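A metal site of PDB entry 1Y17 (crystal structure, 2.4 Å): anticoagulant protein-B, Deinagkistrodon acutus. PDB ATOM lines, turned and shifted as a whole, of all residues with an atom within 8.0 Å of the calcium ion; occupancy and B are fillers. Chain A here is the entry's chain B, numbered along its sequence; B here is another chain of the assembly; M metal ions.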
ATOM      1  N   TYR A   9     -17.628  22.957  28.044  1.00  0.00           N
ATOM      2  CA  TYR A   9     -16.866  24.178  27.952  1.00  0.00           C
ATOM      3  C   TYR A   9     -17.794  25.339  28.289  1.00  0.00           C
ATOM      4  O   TYR A   9     -18.792  25.547  27.598  1.00  0.00           O
ATOM      5  CB  TYR A   9     -16.324  24.367  26.538  1.00  0.00           C
ATOM      6  CG  TYR A   9     -15.597  25.666  26.362  1.00  0.00           C
ATOM      7  CD1 TYR A   9     -14.247  25.790  26.694  1.00  0.00           C
ATOM      8  CD2 TYR A   9     -16.267  26.804  25.903  1.00  0.00           C
ATOM      9  CE1 TYR A   9     -13.581  27.002  26.568  1.00  0.00           C
ATOM     10  CE2 TYR A   9     -15.608  28.037  25.781  1.00  0.00           C
ATOM     11  CZ  TYR A   9     -14.265  28.126  26.118  1.00  0.00           C
ATOM     12  OH  TYR A   9     -13.598  29.323  25.994  1.00  0.00           O
ATOM     13  N   GLU A  10     -17.464  26.075  29.347  1.00  0.00           N
ATOM     14  CA  GLU A  10     -18.257  27.228  29.775  1.00  0.00           C
ATOM     15  C   GLU A  10     -19.776  26.980  29.803  1.00  0.00           C
ATOM     16  O   GLU A  10     -20.536  27.647  29.117  1.00  0.00           O
ATOM     17  CB  GLU A  10     -17.963  28.438  28.873  1.00  0.00           C
ATOM     18  CG  GLU A  10     -16.538  28.948  28.954  1.00  0.00           C
ATOM     19  CD  GLU A  10     -16.159  29.405  30.357  1.00  0.00           C
ATOM     20  OE1 GLU A  10     -16.866  30.276  30.912  1.00  0.00           O
ATOM     21  OE2 GLU A  10     -15.158  28.885  30.909  1.00  0.00           O
ATOM     22  N   HIS A  12     -21.530  24.797  28.477  1.00  0.00           N
ATOM     23  CA  HIS A  12     -22.114  24.241  27.270  1.00  0.00           C
ATOM     24  C   HIS A  12     -21.608  22.836  26.988  1.00  0.00           C
ATOM     25  O   HIS A  12     -20.563  22.417  27.511  1.00  0.00           O
ATOM     26  CB  HIS A  12     -21.833  25.160  26.070  1.00  0.00           C
ATOM     27  CG  HIS A  12     -22.766  26.329  25.979  1.00  0.00           C
ATOM     28  ND1 HIS A  12     -23.066  27.123  27.062  1.00  0.00           N
ATOM     29  CD2 HIS A  12     -23.485  26.828  24.945  1.00  0.00           C
ATOM     30  CE1 HIS A  12     -23.921  28.066  26.700  1.00  0.00           C
ATOM     31  NE2 HIS A  12     -24.193  27.910  25.413  1.00  0.00           N
ATOM     32  N   TYR A  14     -20.711  20.093  23.840  1.00  0.00           N
ATOM     33  CA  TYR A  14     -20.443  19.955  22.418  1.00  0.00           C
ATOM     34  C   TYR A  14     -20.115  18.512  22.011  1.00  0.00           C
ATOM     35  O   TYR A  14     -19.517  17.756  22.778  1.00  0.00           O
ATOM     36  CB  TYR A  14     -19.287  20.858  22.012  1.00  0.00           C
ATOM     37  CG  TYR A  14     -19.419  22.290  22.490  1.00  0.00           C
ATOM     38  CD1 TYR A  14     -19.149  22.637  23.815  1.00  0.00           C
ATOM     39  CD2 TYR A  14     -19.763  23.312  21.606  1.00  0.00           C
ATOM     40  CE1 TYR A  14     -19.219  23.963  24.245  1.00  0.00           C
ATOM     41  CE2 TYR A  14     -19.834  24.635  22.019  1.00  0.00           C
ATOM     42  CZ  TYR A  14     -19.562  24.952  23.331  1.00  0.00           C
ATOM     43  OH  TYR A  14     -19.621  26.267  23.726  1.00  0.00           O
ATOM     44  N   LEU A  39     -26.813  23.123  15.762  1.00  0.00           N
ATOM     45  CA  LEU A  39     -25.467  23.154  15.208  1.00  0.00           C
ATOM     46  C   LEU A  39     -24.728  24.174  16.085  1.00  0.00           C
ATOM     47  O   LEU A  39     -25.341  25.120  16.577  1.00  0.00           O
ATOM     48  CB  LEU A  39     -25.490  23.623  13.755  1.00  0.00           C
ATOM     49  CG  LEU A  39     -25.656  22.519  12.703  1.00  0.00           C
ATOM     50  CD1 LEU A  39     -25.787  23.113  11.310  1.00  0.00           C
ATOM     51  CD2 LEU A  39     -24.461  21.579  12.775  1.00  0.00           C
ATOM     52  N   VAL A  40     -23.435  23.973  16.284  1.00  0.00           N
ATOM     53  CA  VAL A  40     -22.652  24.865  17.129  1.00  0.00           C
ATOM     54  C   VAL A  40     -22.700  26.350  16.724  1.00  0.00           C
ATOM     55  O   VAL A  40     -22.828  26.683  15.530  1.00  0.00           O
ATOM     56  CB  VAL A  40     -21.164  24.421  17.162  1.00  0.00           C
ATOM     57  CG1 VAL A  40     -20.584  24.415  15.749  1.00  0.00           C
ATOM     58  CG2 VAL A  40     -20.353  25.357  18.046  1.00  0.00           C
ATOM     59  N   SER A  41     -22.596  27.224  17.719  1.00  0.00           N
ATOM     60  CA  SER A  41     -22.580  28.678  17.513  1.00  0.00           C
ATOM     61  C   SER A  41     -21.368  29.263  18.257  1.00  0.00           C
ATOM     62  O   SER A  41     -21.049  28.820  19.366  1.00  0.00           O
ATOM     63  CB  SER A  41     -23.858  29.318  18.029  1.00  0.00           C
ATOM     64  OG  SER A  41     -23.957  29.137  19.432  1.00  0.00           O
ATOM     65  N   PHE A  42     -20.693  30.233  17.644  1.00  0.00           N
ATOM     66  CA  PHE A  42     -19.511  30.854  18.251  1.00  0.00           C
ATOM     67  C   PHE A  42     -19.728  32.284  18.734  1.00  0.00           C
ATOM     68  O   PHE A  42     -20.019  33.180  17.940  1.00  0.00           O
ATOM     69  CB  PHE A  42     -18.334  30.854  17.279  1.00  0.00           C
ATOM     70  CG  PHE A  42     -17.882  29.484  16.878  1.00  0.00           C
ATOM     71  CD1 PHE A  42     -17.765  28.472  17.821  1.00  0.00           C
ATOM     72  CD2 PHE A  42     -17.574  29.205  15.554  1.00  0.00           C
ATOM     73  CE1 PHE A  42     -17.346  27.204  17.461  1.00  0.00           C
ATOM     74  CE2 PHE A  42     -17.156  27.935  15.177  1.00  0.00           C
ATOM     75  CZ  PHE A  42     -17.040  26.939  16.136  1.00  0.00           C
ATOM     76  N   GLN A  43     -19.553  32.487  20.026  1.00  0.00           N
ATOM     77  CA  GLN A  43     -19.725  33.806  20.609  1.00  0.00           C
ATOM     78  C   GLN A  43     -18.373  34.413  20.956  1.00  0.00           C
ATOM     79  O   GLN A  43     -18.306  35.558  21.414  1.00  0.00           O
ATOM     80  CB  GLN A  43     -20.595  33.714  21.867  1.00  0.00           C
ATOM     81  CG  GLN A  43     -22.082  33.931  21.631  1.00  0.00           C
ATOM     82  CD  GLN A  43     -22.667  33.019  20.560  1.00  0.00           C
ATOM     83  OE1 GLN A  43     -22.513  31.794  20.608  1.00  0.00           O
ATOM     84  NE2 GLN A  43     -23.347  33.623  19.586  1.00  0.00           N
ATOM     85  N   SER A  44     -17.309  33.652  20.755  1.00  0.00           N
ATOM     86  CA  SER A  44     -15.968  34.145  21.060  1.00  0.00           C
ATOM     87  C   SER A  44     -14.870  33.305  20.436  1.00  0.00           C
ATOM     88  O   SER A  44     -15.110  32.188  19.962  1.00  0.00           O
ATOM     89  CB  SER A  44     -15.757  34.195  22.582  1.00  0.00           C
ATOM     90  OG  SER A  44     -15.692  32.889  23.136  1.00  0.00           O
ATOM     91  N   GLU A  47     -13.960  30.069  22.499  1.00  0.00           N
ATOM     92  CA  GLU A  47     -14.918  29.002  22.237  1.00  0.00           C
ATOM     93  C   GLU A  47     -14.617  28.353  20.889  1.00  0.00           C
ATOM     94  O   GLU A  47     -14.663  27.131  20.756  1.00  0.00           O
ATOM     95  CB  GLU A  47     -16.347  29.563  22.225  1.00  0.00           C
ATOM     96  CG  GLU A  47     -17.395  28.593  21.688  1.00  0.00           C
ATOM     97  CD  GLU A  47     -18.822  29.107  21.805  1.00  0.00           C
ATOM     98  OE1 GLU A  47     -19.054  30.276  21.454  1.00  0.00           O
ATOM     99  OE2 GLU A  47     -19.712  28.353  22.232  1.00  0.00           O
ATOM    100  N   VAL A  51     -13.721  24.374  20.112  1.00  0.00           N
ATOM    101  CA  VAL A  51     -14.435  23.463  19.218  1.00  0.00           C
ATOM    102  C   VAL A  51     -13.525  22.919  18.122  1.00  0.00           C
ATOM    103  O   VAL A  51     -13.628  21.746  17.752  1.00  0.00           O
ATOM    104  CB  VAL A  51     -15.660  24.161  18.585  1.00  0.00           C
ATOM    105  CG1 VAL A  51     -16.416  23.189  17.703  1.00  0.00           C
ATOM    106  CG2 VAL A  51     -16.570  24.705  19.682  1.00  0.00           C
ATOM    107  N   GLU A 120     -24.421  21.422  19.777  1.00  0.00           N
ATOM    108  CA  GLU A 120     -24.230  22.105  21.044  1.00  0.00           C
ATOM    109  C   GLU A 120     -25.546  22.407  21.755  1.00  0.00           C
ATOM    110  O   GLU A 120     -26.599  22.507  21.112  1.00  0.00           O
ATOM    111  CB  GLU A 120     -23.443  23.400  20.788  1.00  0.00           C
ATOM    112  CG  GLU A 120     -23.778  24.557  21.713  1.00  0.00           C
ATOM    113  CD  GLU A 120     -22.965  25.806  21.410  1.00  0.00           C
ATOM    114  OE1 GLU A 120     -22.800  26.138  20.221  1.00  0.00           O
ATOM    115  OE2 GLU A 120     -22.511  26.472  22.365  1.00  0.00           O
ATOM    116  N   PHE A 121     -25.497  22.533  23.066  1.00  0.00           N
ATOM    117  CA  PHE A 121     -26.684  22.866  23.847  1.00  0.00           C
ATOM    118  C   PHE A 121     -26.261  23.388  25.214  1.00  0.00           C
ATOM    119  O   PHE A 121     -25.140  23.127  25.660  1.00  0.00           O
ATOM    120  CB  PHE A 121     -27.633  21.659  23.989  1.00  0.00           C
ATOM    121  CG  PHE A 121     -27.094  20.517  24.824  1.00  0.00           C
ATOM    122  CD1 PHE A 121     -27.060  20.608  26.211  1.00  0.00           C
ATOM    123  CD2 PHE A 121     -26.662  19.334  24.218  1.00  0.00           C
ATOM    124  CE1 PHE A 121     -26.607  19.535  26.990  1.00  0.00           C
ATOM    125  CE2 PHE A 121     -26.211  18.259  24.980  1.00  0.00           C
ATOM    126  CZ  PHE A 121     -26.180  18.357  26.372  1.00  0.00           C
ATOM    127  N   TRP B  83     -28.156  32.679  14.553  1.00  0.00           N
ATOM    128  CA  TRP B  83     -27.653  31.319  14.458  1.00  0.00           C
ATOM    129  C   TRP B  83     -28.876  30.423  14.539  1.00  0.00           C
ATOM    130  O   TRP B  83     -29.974  30.875  14.878  1.00  0.00           O
ATOM    131  CB  TRP B  83     -26.738  31.006  15.635  1.00  0.00           C
ATOM    132  CG  TRP B  83     -25.494  31.809  15.647  1.00  0.00           C
ATOM    133  CD1 TRP B  83     -25.343  33.075  16.141  1.00  0.00           C
ATOM    134  CD2 TRP B  83     -24.220  31.408  15.156  1.00  0.00           C
ATOM    135  NE1 TRP B  83     -24.040  33.483  15.987  1.00  0.00           N
ATOM    136  CE2 TRP B  83     -23.327  32.485  15.385  1.00  0.00           C
ATOM    137  CE3 TRP B  83     -23.738  30.251  14.537  1.00  0.00           C
ATOM    138  CZ2 TRP B  83     -21.981  32.425  15.018  1.00  0.00           C
ATOM    139  CZ3 TRP B  83     -22.403  30.183  14.172  1.00  0.00           C
ATOM    140  CH2 TRP B  83     -21.535  31.273  14.418  1.00  0.00           C
ATOM    141  N   ASP B  85     -29.484  28.394  16.723  1.00  0.00           N
ATOM    142  CA  ASP B  85     -29.925  28.277  18.104  1.00  0.00           C
ATOM    143  C   ASP B  85     -30.694  29.502  18.567  1.00  0.00           C
ATOM    144  O   ASP B  85     -31.060  29.595  19.733  1.00  0.00           O
ATOM    145  CB  ASP B  85     -28.741  28.016  19.053  1.00  0.00           C
ATOM    146  CG  ASP B  85     -27.767  29.172  19.103  1.00  0.00           C
ATOM    147  OD1 ASP B  85     -28.158  30.332  18.822  1.00  0.00           O
ATOM    148  OD2 ASP B  85     -26.593  28.911  19.440  1.00  0.00           O
ATOM    149  N   SER B  87     -29.691  32.656  18.937  1.00  0.00           N
ATOM    150  CA  SER B  87     -28.906  33.784  19.446  1.00  0.00           C
ATOM    151  C   SER B  87     -28.482  34.676  18.293  1.00  0.00           C
ATOM    152  O   SER B  87     -28.419  34.241  17.152  1.00  0.00           O
ATOM    153  CB  SER B  87     -27.664  33.285  20.162  1.00  0.00           C
ATOM    154  OG  SER B  87     -26.767  32.677  19.244  1.00  0.00           O
HETATM  155 CA    CA M   1     -22.188  28.833  21.449  1.00  0.00          CA
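The side-chain hydroxyl of Ser 41 lies close to the side-chain amide oxygen of Gln 43, 3.2 Å away. OE2 of Glu 120 sits close to OH of Tyr 14 (3.2 Å). N of Glu 47 sits at hydrogen-bond distance from OG of Ser 44, 3.4 Å away. N of Gln 43 is in hydrogen-bond range of OE1 of Glu 47 (2.7 Å). The side-chain hydroxyl of Tyr 14 lies close to the side-chain carboxylate of Glu 47 (2.6 Å). OG of Ser 41 lies close to OD2 of Asp 85 of chain B (2.6 Å).
Four residues have an atom within 4 Å of the calcium ion: Ser 41, Gln 43, Glu 47 and Glu 120. The nearest printed residue that does not touch the calcium ion is His 12 (4.2 Å).
The backbone carbonyl oxygen (O) of Ser 41 binds the calcium ion (2.4 Å). OE2 of Glu 120 binds the calcium ion (2.6 Å). The calcium ion is bound by the side-chain carboxylate (OE2) of Glu 47 (2.6 Å). The side-chain hydroxyl (OG) of Ser 41 binds the calcium ion, at 2.7 Å. Slightly farther from the calcium ion lies OE1 of Glu 120 (3.0 Å). Slightly farther from the calcium ion lies OE1 of Gln 43 (3.1 Å).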
